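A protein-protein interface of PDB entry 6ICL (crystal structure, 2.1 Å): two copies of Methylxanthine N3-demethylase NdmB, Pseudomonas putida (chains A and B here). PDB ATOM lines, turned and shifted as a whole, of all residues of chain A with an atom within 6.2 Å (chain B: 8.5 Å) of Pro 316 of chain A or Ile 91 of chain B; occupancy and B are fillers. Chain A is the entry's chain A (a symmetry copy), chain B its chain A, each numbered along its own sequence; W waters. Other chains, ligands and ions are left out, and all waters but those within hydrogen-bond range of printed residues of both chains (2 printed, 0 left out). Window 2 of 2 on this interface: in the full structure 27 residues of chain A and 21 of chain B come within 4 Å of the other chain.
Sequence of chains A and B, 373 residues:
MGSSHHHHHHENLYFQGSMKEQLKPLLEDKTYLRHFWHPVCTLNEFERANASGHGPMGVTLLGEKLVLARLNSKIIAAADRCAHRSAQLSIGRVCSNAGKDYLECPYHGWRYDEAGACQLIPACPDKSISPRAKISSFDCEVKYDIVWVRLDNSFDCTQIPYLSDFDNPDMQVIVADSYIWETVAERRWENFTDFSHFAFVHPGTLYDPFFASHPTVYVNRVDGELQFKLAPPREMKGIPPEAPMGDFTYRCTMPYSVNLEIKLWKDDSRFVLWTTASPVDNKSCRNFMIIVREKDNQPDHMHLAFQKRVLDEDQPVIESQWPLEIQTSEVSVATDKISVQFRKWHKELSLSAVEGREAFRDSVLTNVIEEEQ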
ATOM      1  N   LEU A 311      -8.467  -8.291  24.482  1.00  0.00           N
ATOM      2  CA  LEU A 311      -7.207  -8.646  23.827  1.00  0.00           C
ATOM      3  C   LEU A 311      -6.205  -9.200  24.821  1.00  0.00           C
ATOM      4  O   LEU A 311      -5.505 -10.182  24.538  1.00  0.00           O
ATOM      5  CB  LEU A 311      -6.621  -7.418  23.125  1.00  0.00           C
ATOM      6  CG  LEU A 311      -7.372  -6.864  21.912  1.00  0.00           C
ATOM      7  CD1 LEU A 311      -6.746  -5.523  21.492  1.00  0.00           C
ATOM      8  CD2 LEU A 311      -7.321  -7.876  20.757  1.00  0.00           C
ATOM      9  N   ASP A 312      -6.137  -8.603  26.008  1.00  0.00           N
ATOM     10  CA  ASP A 312      -5.159  -9.076  26.981  1.00  0.00           C
ATOM     11  C   ASP A 312      -5.522 -10.440  27.546  1.00  0.00           C
ATOM     12  O   ASP A 312      -4.625 -11.150  28.008  1.00  0.00           O
ATOM     13  CB  ASP A 312      -4.991  -8.073  28.131  1.00  0.00           C
ATOM     14  CG  ASP A 312      -4.202  -6.841  27.716  1.00  0.00           C
ATOM     15  OD1 ASP A 312      -3.426  -6.905  26.724  1.00  0.00           O
ATOM     16  OD2 ASP A 312      -4.376  -5.803  28.394  1.00  0.00           O
ATOM     17  N   GLU A 313      -6.801 -10.834  27.500  1.00  0.00           N
ATOM     18  CA  GLU A 313      -7.156 -12.207  27.878  1.00  0.00           C
ATOM     19  C   GLU A 313      -6.743 -13.210  26.798  1.00  0.00           C
ATOM     20  O   GLU A 313      -6.185 -14.265  27.108  1.00  0.00           O
ATOM     21  CB  GLU A 313      -8.658 -12.291  28.172  1.00  0.00           C
ATOM     22  CG  GLU A 313      -9.036 -11.515  29.414  1.00  0.00           C
ATOM     23  CD  GLU A 313     -10.527 -11.336  29.566  1.00  0.00           C
ATOM     24  OE1 GLU A 313     -11.275 -11.504  28.577  1.00  0.00           O
ATOM     25  OE2 GLU A 313     -10.946 -11.009  30.686  1.00  0.00           O
ATOM     26  N   ASP A 314      -6.969 -12.881  25.526  1.00  0.00           N
ATOM     27  CA  ASP A 314      -6.585 -13.778  24.436  1.00  0.00           C
ATOM     28  C   ASP A 314      -5.072 -13.896  24.293  1.00  0.00           C
ATOM     29  O   ASP A 314      -4.557 -14.980  23.987  1.00  0.00           O
ATOM     30  CB  ASP A 314      -7.166 -13.279  23.117  1.00  0.00           C
ATOM     31  CG  ASP A 314      -8.655 -13.589  22.954  1.00  0.00           C
ATOM     32  OD1 ASP A 314      -9.095 -14.725  23.229  1.00  0.00           O
ATOM     33  OD2 ASP A 314      -9.379 -12.691  22.517  1.00  0.00           O
ATOM     34  N   GLN A 315      -4.343 -12.784  24.450  1.00  0.00           N
ATOM     35  CA  GLN A 315      -2.948 -12.732  24.022  1.00  0.00           C
ATOM     36  C   GLN A 315      -2.084 -13.876  24.558  1.00  0.00           C
ATOM     37  O   GLN A 315      -1.440 -14.559  23.751  1.00  0.00           O
ATOM     38  CB  GLN A 315      -2.317 -11.383  24.404  1.00  0.00           C
ATOM     39  CG  GLN A 315      -0.855 -11.291  23.889  1.00  0.00           C
ATOM     40  CD  GLN A 315      -0.231  -9.902  24.059  1.00  0.00           C
ATOM     41  OE1 GLN A 315      -0.818  -9.048  24.706  1.00  0.00           O
ATOM     42  NE2 GLN A 315       0.955  -9.674  23.449  1.00  0.00           N
ATOM     43  N   PRO A 316      -2.005 -14.132  25.865  1.00  0.00           N
ATOM     44  CA  PRO A 316      -1.092 -15.198  26.314  1.00  0.00           C
ATOM     45  C   PRO A 316      -1.542 -16.592  25.898  1.00  0.00           C
ATOM     46  O   PRO A 316      -0.697 -17.473  25.719  1.00  0.00           O
ATOM     47  CB  PRO A 316      -1.084 -15.038  27.838  1.00  0.00           C
ATOM     48  CG  PRO A 316      -2.405 -14.365  28.140  1.00  0.00           C
ATOM     49  CD  PRO A 316      -2.645 -13.441  26.998  1.00  0.00           C
ATOM     50  N   VAL A 317      -2.843 -16.822  25.717  1.00  0.00           N
ATOM     51  CA  VAL A 317      -3.292 -18.138  25.265  1.00  0.00           C
ATOM     52  C   VAL A 317      -2.891 -18.363  23.814  1.00  0.00           C
ATOM     53  O   VAL A 317      -2.313 -19.400  23.460  1.00  0.00           O
ATOM     54  CB  VAL A 317      -4.810 -18.282  25.473  1.00  0.00           C
ATOM     55  CG1 VAL A 317      -5.298 -19.649  24.955  1.00  0.00           C
ATOM     56  CG2 VAL A 317      -5.134 -18.105  26.963  1.00  0.00           C
ATOM     57  N   ILE A 318      -3.122 -17.362  22.965  1.00  0.00           N
ATOM     58  CA  ILE A 318      -2.814 -17.503  21.543  1.00  0.00           C
ATOM     59  C   ILE A 318      -1.308 -17.549  21.328  1.00  0.00           C
ATOM     60  O   ILE A 318      -0.806 -18.310  20.482  1.00  0.00           O
ATOM     61  CB  ILE A 318      -3.469 -16.364  20.733  1.00  0.00           C
ATOM     62  CG1 ILE A 318      -4.974 -16.599  20.504  1.00  0.00           C
ATOM     63  CG2 ILE A 318      -2.860 -16.277  19.361  1.00  0.00           C
ATOM     64  CD1 ILE A 318      -5.718 -17.309  21.578  1.00  0.00           C
ATOM     65  N   GLU A 319      -0.558 -16.727  22.065  1.00  0.00           N
ATOM     66  CA  GLU A 319       0.897 -16.793  21.945  1.00  0.00           C
ATOM     67  C   GLU A 319       1.469 -18.111  22.471  1.00  0.00           C
ATOM     68  O   GLU A 319       2.604 -18.453  22.136  1.00  0.00           O
ATOM     69  CB  GLU A 319       1.533 -15.595  22.666  1.00  0.00           C
ATOM     70  CG  GLU A 319       1.283 -14.278  21.880  1.00  0.00           C
ATOM     71  CD  GLU A 319       1.948 -13.039  22.485  1.00  0.00           C
ATOM     72  OE1 GLU A 319       2.414 -13.100  23.641  1.00  0.00           O
ATOM     73  OE2 GLU A 319       1.989 -11.988  21.798  1.00  0.00           O
ATOM     74  N   SER A 320       0.706 -18.874  23.263  1.00  0.00           N
ATOM     75  CA  SER A 320       1.180 -20.179  23.703  1.00  0.00           C
ATOM     76  C   SER A 320       1.034 -21.249  22.630  1.00  0.00           C
ATOM     77  O   SER A 320       1.610 -22.340  22.778  1.00  0.00           O
ATOM     78  CB  SER A 320       0.431 -20.629  24.954  1.00  0.00           C
ATOM     79  OG  SER A 320      -0.784 -21.281  24.585  1.00  0.00           O
ATOM     80  N   GLN A 321       0.285 -20.975  21.567  1.00  0.00           N
ATOM     81  CA  GLN A 321       0.039 -21.990  20.555  1.00  0.00           C
ATOM     82  C   GLN A 321       1.317 -22.287  19.785  1.00  0.00           C
ATOM     83  O   GLN A 321       1.945 -21.377  19.236  1.00  0.00           O
ATOM     84  CB  GLN A 321      -1.049 -21.537  19.591  1.00  0.00           C
ATOM     85  CG  GLN A 321      -2.465 -21.503  20.170  1.00  0.00           C
ATOM     86  CD  GLN A 321      -3.464 -21.022  19.124  1.00  0.00           C
ATOM     87  OE1 GLN A 321      -3.658 -19.826  18.946  1.00  0.00           O
ATOM     88  NE2 GLN A 321      -4.059 -21.957  18.389  1.00  0.00           N
ATOM     89  N   ALA B  49       4.210 -23.799  41.537  1.00  0.00           N
ATOM     90  CA  ALA B  49       4.063 -23.333  40.163  1.00  0.00           C
ATOM     91  C   ALA B  49       2.672 -22.789  39.843  1.00  0.00           C
ATOM     92  O   ALA B  49       2.514 -22.074  38.852  1.00  0.00           O
ATOM     93  CB  ALA B  49       4.365 -24.479  39.205  1.00  0.00           C
ATOM     94  N   ASN B  50       1.655 -23.136  40.623  1.00  0.00           N
ATOM     95  CA  ASN B  50       0.288 -22.737  40.322  1.00  0.00           C
ATOM     96  C   ASN B  50      -0.402 -22.564  41.667  1.00  0.00           C
ATOM     97  O   ASN B  50      -0.140 -23.343  42.584  1.00  0.00           O
ATOM     98  CB  ASN B  50      -0.415 -23.799  39.443  1.00  0.00           C
ATOM     99  CG  ASN B  50      -1.842 -23.406  39.048  1.00  0.00           C
ATOM    100  OD1 ASN B  50      -2.763 -23.452  39.863  1.00  0.00           O
ATOM    101  ND2 ASN B  50      -2.033 -23.051  37.783  1.00  0.00           N
ATOM    102  N   GLY B  55      -0.636 -27.764  40.090  1.00  0.00           N
ATOM    103  CA  GLY B  55      -0.335 -27.463  38.698  1.00  0.00           C
ATOM    104  C   GLY B  55      -1.543 -26.857  38.011  1.00  0.00           C
ATOM    105  O   GLY B  55      -2.477 -26.427  38.678  1.00  0.00           O
ATOM    106  N   PRO B  56      -1.545 -26.823  36.677  1.00  0.00           N
ATOM    107  CA  PRO B  56      -0.521 -27.383  35.787  1.00  0.00           C
ATOM    108  C   PRO B  56       0.774 -26.556  35.779  1.00  0.00           C
ATOM    109  O   PRO B  56       0.763 -25.389  36.180  1.00  0.00           O
ATOM    110  CB  PRO B  56      -1.213 -27.377  34.422  1.00  0.00           C
ATOM    111  CG  PRO B  56      -2.162 -26.164  34.498  1.00  0.00           C
ATOM    112  CD  PRO B  56      -2.628 -26.140  35.941  1.00  0.00           C
ATOM    113  N   MET B  57       1.882 -27.181  35.385  1.00  0.00           N
ATOM    114  CA  MET B  57       3.186 -26.529  35.382  1.00  0.00           C
ATOM    115  C   MET B  57       3.905 -26.963  34.117  1.00  0.00           C
ATOM    116  O   MET B  57       3.676 -28.072  33.612  1.00  0.00           O
ATOM    117  CB  MET B  57       4.018 -26.883  36.651  1.00  0.00           C
ATOM    118  CG  MET B  57       5.417 -27.546  36.419  1.00  0.00           C
ATOM    119  SD  MET B  57       6.475 -27.391  37.846  1.00  0.00           S
ATOM    120  CE  MET B  57       7.984 -26.655  37.246  1.00  0.00           C
ATOM    121  N   GLY B  58       4.757 -26.084  33.599  1.00  0.00           N
ATOM    122  CA  GLY B  58       5.561 -26.379  32.418  1.00  0.00           C
ATOM    123  C   GLY B  58       7.000 -26.695  32.807  1.00  0.00           C
ATOM    124  O   GLY B  58       7.564 -26.049  33.686  1.00  0.00           O
ATOM    125  N   LEU B  66       6.784 -30.254  28.291  1.00  0.00           N
ATOM    126  CA  LEU B  66       5.898 -31.147  29.027  1.00  0.00           C
ATOM    127  C   LEU B  66       5.033 -30.320  29.956  1.00  0.00           C
ATOM    128  O   LEU B  66       5.454 -29.259  30.428  1.00  0.00           O
ATOM    129  CB  LEU B  66       6.688 -32.164  29.902  1.00  0.00           C
ATOM    130  CG  LEU B  66       7.815 -33.000  29.250  1.00  0.00           C
ATOM    131  CD1 LEU B  66       8.429 -33.955  30.274  1.00  0.00           C
ATOM    132  CD2 LEU B  66       7.308 -33.770  28.057  1.00  0.00           C
ATOM    133  N   VAL B  67       3.843 -30.833  30.261  1.00  0.00           N
ATOM    134  CA  VAL B  67       3.000 -30.269  31.311  1.00  0.00           C
ATOM    135  C   VAL B  67       2.909 -31.281  32.444  1.00  0.00           C
ATOM    136  O   VAL B  67       2.754 -32.486  32.203  1.00  0.00           O
ATOM    137  CB  VAL B  67       1.605 -29.881  30.779  1.00  0.00           C
ATOM    138  CG1 VAL B  67       0.939 -31.067  30.048  1.00  0.00           C
ATOM    139  CG2 VAL B  67       0.725 -29.360  31.916  1.00  0.00           C
ATOM    140  N   LEU B  68       3.069 -30.802  33.672  1.00  0.00           N
ATOM    141  CA  LEU B  68       2.840 -31.576  34.878  1.00  0.00           C
ATOM    142  C   LEU B  68       1.537 -31.110  35.511  1.00  0.00           C
ATOM    143  O   LEU B  68       1.276 -29.904  35.598  1.00  0.00           O
ATOM    144  CB  LEU B  68       3.988 -31.398  35.881  1.00  0.00           C
ATOM    145  CG  LEU B  68       5.404 -31.710  35.364  1.00  0.00           C
ATOM    146  CD1 LEU B  68       6.438 -31.482  36.449  1.00  0.00           C
ATOM    147  CD2 LEU B  68       5.500 -33.151  34.826  1.00  0.00           C
ATOM    148  N   ASP B  80       3.024 -30.757  26.330  1.00  0.00           N
ATOM    149  CA  ASP B  80       2.447 -29.443  26.632  1.00  0.00           C
ATOM    150  C   ASP B  80       1.862 -28.805  25.371  1.00  0.00           C
ATOM    151  O   ASP B  80       2.258 -27.719  24.921  1.00  0.00           O
ATOM    152  CB  ASP B  80       3.496 -28.537  27.262  1.00  0.00           C
ATOM    153  CG  ASP B  80       2.875 -27.300  27.916  1.00  0.00           C
ATOM    154  OD1 ASP B  80       1.623 -27.268  28.092  1.00  0.00           O
ATOM    155  OD2 ASP B  80       3.652 -26.368  28.254  1.00  0.00           O
ATOM    156  N   ALA B  87      -2.603 -25.051  21.900  1.00  0.00           N
ATOM    157  CA  ALA B  87      -2.330 -24.225  23.076  1.00  0.00           C
ATOM    158  C   ALA B  87      -1.523 -24.998  24.124  1.00  0.00           C
ATOM    159  O   ALA B  87      -1.540 -26.230  24.173  1.00  0.00           O
ATOM    160  CB  ALA B  87      -3.637 -23.720  23.681  1.00  0.00           C
ATOM    161  N   GLN B  88      -0.795 -24.261  24.974  1.00  0.00           N
ATOM    162  CA  GLN B  88      -0.058 -24.900  26.056  1.00  0.00           C
ATOM    163  C   GLN B  88      -0.996 -25.276  27.192  1.00  0.00           C
ATOM    164  O   GLN B  88      -1.615 -24.402  27.816  1.00  0.00           O
ATOM    165  CB  GLN B  88       1.044 -23.994  26.582  1.00  0.00           C
ATOM    166  CG  GLN B  88       2.323 -24.115  25.771  1.00  0.00           C
ATOM    167  CD  GLN B  88       3.420 -23.247  26.356  1.00  0.00           C
ATOM    168  OE1 GLN B  88       3.438 -22.044  26.130  1.00  0.00           O
ATOM    169  NE2 GLN B  88       4.321 -23.847  27.128  1.00  0.00           N
ATOM    170  N   LEU B  89      -1.069 -26.579  27.493  1.00  0.00           N
ATOM    171  CA  LEU B  89      -1.882 -27.031  28.610  1.00  0.00           C
ATOM    172  C   LEU B  89      -1.338 -26.524  29.937  1.00  0.00           C
ATOM    173  O   LEU B  89      -2.105 -26.370  30.902  1.00  0.00           O
ATOM    174  CB  LEU B  89      -1.978 -28.574  28.590  1.00  0.00           C
ATOM    175  CG  LEU B  89      -2.576 -29.132  27.282  1.00  0.00           C
ATOM    176  CD1 LEU B  89      -2.457 -30.647  27.205  1.00  0.00           C
ATOM    177  CD2 LEU B  89      -4.042 -28.732  27.147  1.00  0.00           C
ATOM    178  N   SER B  90      -0.034 -26.205  29.997  1.00  0.00           N
ATOM    179  CA  SER B  90       0.591 -25.830  31.268  1.00  0.00           C
ATOM    180  C   SER B  90       0.107 -24.485  31.793  1.00  0.00           C
ATOM    181  O   SER B  90       0.357 -24.170  32.967  1.00  0.00           O
ATOM    182  CB  SER B  90       2.123 -25.815  31.129  1.00  0.00           C
ATOM    183  OG  SER B  90       2.543 -24.874  30.134  1.00  0.00           O
ATOM    184  N   ILE B  91      -0.556 -23.685  30.959  1.00  0.00           N
ATOM    185  CA  ILE B  91      -1.221 -22.469  31.424  1.00  0.00           C
ATOM    186  C   ILE B  91      -2.743 -22.660  31.511  1.00  0.00           C
ATOM    187  O   ILE B  91      -3.483 -21.684  31.576  1.00  0.00           O
ATOM    188  CB  ILE B  91      -0.858 -21.238  30.567  1.00  0.00           C
ATOM    189  CG1 ILE B  91      -1.442 -21.317  29.155  1.00  0.00           C
ATOM    190  CG2 ILE B  91       0.669 -21.040  30.510  1.00  0.00           C
ATOM    191  CD1 ILE B  91      -1.122 -20.055  28.278  1.00  0.00           C
ATOM    192  N   GLY B  92      -3.220 -23.906  31.521  1.00  0.00           N
ATOM    193  CA  GLY B  92      -4.629 -24.129  31.789  1.00  0.00           C
ATOM    194  C   GLY B  92      -4.886 -24.383  33.257  1.00  0.00           C
ATOM    195  O   GLY B  92      -4.285 -23.752  34.130  1.00  0.00           O
ATOM    196  N   ARG B  93      -5.760 -25.330  33.568  1.00  0.00           N
ATOM    197  CA  ARG B  93      -6.123 -25.514  34.961  1.00  0.00           C
ATOM    198  C   ARG B  93      -6.508 -26.965  35.196  1.00  0.00           C
ATOM    199  O   ARG B  93      -7.011 -27.645  34.296  1.00  0.00           O
ATOM    200  CB  ARG B  93      -7.278 -24.589  35.377  1.00  0.00           C
ATOM    201  CG  ARG B  93      -8.655 -25.028  34.876  1.00  0.00           C
ATOM    202  CD  ARG B  93      -9.743 -24.070  35.393  1.00  0.00           C
ATOM    203  NE  ARG B  93     -11.097 -24.498  35.026  1.00  0.00           N
ATOM    204  CZ  ARG B  93     -11.979 -25.018  35.878  1.00  0.00           C
ATOM    205  NH1 ARG B  93     -11.659 -25.177  37.165  1.00  0.00           N
ATOM    206  NH2 ARG B  93     -13.187 -25.375  35.443  1.00  0.00           N
ATOM    207  N   VAL B  94      -6.251 -27.424  36.418  1.00  0.00           N
ATOM    208  CA  VAL B  94      -6.774 -28.698  36.893  1.00  0.00           C
ATOM    209  C   VAL B  94      -8.203 -28.449  37.369  1.00  0.00           C
ATOM    210  O   VAL B  94      -8.443 -27.577  38.201  1.00  0.00           O
ATOM    211  CB  VAL B  94      -5.913 -29.263  38.029  1.00  0.00           C
ATOM    212  CG1 VAL B  94      -6.653 -30.415  38.719  1.00  0.00           C
ATOM    213  CG2 VAL B  94      -4.574 -29.720  37.484  1.00  0.00           C
ATOM    214  N   LEU B 103      -7.152 -32.225  33.246  1.00  0.00           N
ATOM    215  CA  LEU B 103      -6.328 -31.102  32.822  1.00  0.00           C
ATOM    216  C   LEU B 103      -7.076 -30.381  31.709  1.00  0.00           C
ATOM    217  O   LEU B 103      -7.283 -30.934  30.622  1.00  0.00           O
ATOM    218  CB  LEU B 103      -4.958 -31.588  32.374  1.00  0.00           C
ATOM    219  CG  LEU B 103      -4.033 -30.560  31.719  1.00  0.00           C
ATOM    220  CD1 LEU B 103      -3.655 -29.486  32.712  1.00  0.00           C
ATOM    221  CD2 LEU B 103      -2.812 -31.326  31.263  1.00  0.00           C
ATOM    222  N   GLU B 104      -7.501 -29.161  31.986  1.00  0.00           N
ATOM    223  CA  GLU B 104      -8.337 -28.410  31.065  1.00  0.00           C
ATOM    224  C   GLU B 104      -7.478 -27.471  30.231  1.00  0.00           C
ATOM    225  O   GLU B 104      -6.673 -26.723  30.782  1.00  0.00           O
ATOM    226  CB  GLU B 104      -9.390 -27.611  31.831  1.00  0.00           C
ATOM    227  CG  GLU B 104     -10.313 -26.830  30.936  1.00  0.00           C
ATOM    228  CD  GLU B 104     -11.270 -25.952  31.729  1.00  0.00           C
ATOM    229  OE1 GLU B 104     -10.802 -25.026  32.421  1.00  0.00           O
ATOM    230  OE2 GLU B 104     -12.486 -26.212  31.683  1.00  0.00           O
ATOM    231  N   CYS B 105      -7.663 -27.497  28.918  1.00  0.00           N
ATOM    232  CA  CYS B 105      -6.915 -26.580  28.061  1.00  0.00           C
ATOM    233  C   CYS B 105      -7.372 -25.138  28.307  1.00  0.00           C
ATOM    234  O   CYS B 105      -8.557 -24.896  28.545  1.00  0.00           O
ATOM    235  CB  CYS B 105      -7.100 -26.949  26.596  1.00  0.00           C
ATOM    236  SG  CYS B 105      -6.245 -25.804  25.433  1.00  0.00           S
ATOM    237  N   PRO B 106      -6.451 -24.153  28.268  1.00  0.00           N
ATOM    238  CA  PRO B 106      -6.867 -22.752  28.490  1.00  0.00           C
ATOM    239  C   PRO B 106      -7.650 -22.163  27.342  1.00  0.00           C
ATOM    240  O   PRO B 106      -8.235 -21.078  27.505  1.00  0.00           O
ATOM    241  CB  PRO B 106      -5.529 -22.009  28.656  1.00  0.00           C
ATOM    242  CG  PRO B 106      -4.576 -22.798  27.814  1.00  0.00           C
ATOM    243  CD  PRO B 106      -4.990 -24.256  28.064  1.00  0.00           C
ATOM    244  N   TYR B 107      -7.657 -22.811  26.177  1.00  0.00           N
ATOM    245  CA  TYR B 107      -8.183 -22.145  24.991  1.00  0.00           C
ATOM    246  C   TYR B 107      -9.659 -22.496  24.763  1.00  0.00           C
ATOM    247  O   TYR B 107     -10.543 -21.654  24.975  1.00  0.00           O
ATOM    248  CB  TYR B 107      -7.304 -22.488  23.783  1.00  0.00           C
ATOM    249  CG  TYR B 107      -7.447 -21.546  22.604  1.00  0.00           C
ATOM    250  CD1 TYR B 107      -8.406 -20.529  22.606  1.00  0.00           C
ATOM    251  CD2 TYR B 107      -6.624 -21.683  21.474  1.00  0.00           C
ATOM    252  CE1 TYR B 107      -8.548 -19.688  21.507  1.00  0.00           C
ATOM    253  CE2 TYR B 107      -6.758 -20.832  20.364  1.00  0.00           C
ATOM    254  CZ  TYR B 107      -7.726 -19.844  20.396  1.00  0.00           C
ATOM    255  OH  TYR B 107      -7.862 -18.992  19.319  1.00  0.00           O
HETATM  256  O   HOH W   1      -5.817 -18.986  17.552  1.00  0.00           O
HETATM  257  O   HOH W   2       4.703 -22.021  23.209  1.00  0.00           O
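OG of Ser 320 of chain A is in hydrogen-bond range of N of Gln 88 of chain B, at 3.0 Å.
OD2 of Asp 80 of chain B sits at hydrogen-bond distance from NE2 of Gln 88 of chain B (2.8 Å). The side-chain sulfur of Cys 105 of chain B sits close to the backbone NH of Tyr 107 of chain B (3.4 Å). The side-chain hydroxyl (OG) of Ser 320 of chain A sits at hydrogen-bond distance from the backbone carbonyl oxygen (O) of Val 317 of chain A.
Pro 316 of chain A touches Ile 91 of chain B. Tyr 107 of chain B touches Val 317 of chain A (CB to CG1, 3.7 Å). Ile 318 of chain A touches Tyr 107 of chain B (CD1 to CZ, 3.4 Å). Ser 320 of chain A touches Ala 87 of chain B. Ser 320 of chain A touches Ile 91 of chain B (CB to CD1, 3.7 Å). N of Ala 87 of chain B touches CG of Gln 321 of chain A (3.9 Å). Gln 321 of chain A touches Tyr 107 of chain B (CD to CE2, 3.5 Å).
Pro 316 of chain A touches just one residue of chain B: Ile 91. Of the printed residues of chain B, Val 317 of chain A touches Tyr 107. Of the printed residues of chain B, Ser 320 of chain A touches Ala 87 (3.7 Å), Gln 88 (3.0 Å) and Ile 91 (3.7 Å). Printed residues of chain A within 4 Å of Ala 87 of chain B: Ser 320 and Gln 321. Printed residues of chain A within 4 Å of Gln 88 of chain B: Ser 320. Ile 91 of chain B touches two residues of chain A. The nearest printed residue of chain B that does not touch Ile 318 of chain A is Ile 91 of chain B (6.3 Å).
Of the 11 printed residues of chain A, 5 touch a printed residue of chain B. Hydrophobic or aromatic side chains of chain A that line the printed part of chain B: Val 317 and Ile 318. Hydrophobic or aromatic side chains of chain B within 4 Å of the printed part of chain A: Ala 87, Ile 91 and Tyr 107. Among the printed residues, 8 pairs touch across the chains. Among the printed residues, no Asp or Glu carboxylate lies within 4 Å of a Lys or Arg side-chain nitrogen of the other chain.
No position is printed for both chains. Of the 8 pairs that touch across the chains among the printed residues, none has its exchanged pair printed and touching as well.
Water W1 lies within hydrogen-bond range of OH of Tyr 107 of chain B (2.7 Å) and OE1 of Gln 321 of chain A (2.7 Å). Water W2 lies within hydrogen-bond range of O of Ser 320 of chain A (3.1 Å) and OE1 of Gln 88 of chain B (3.2 Å).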
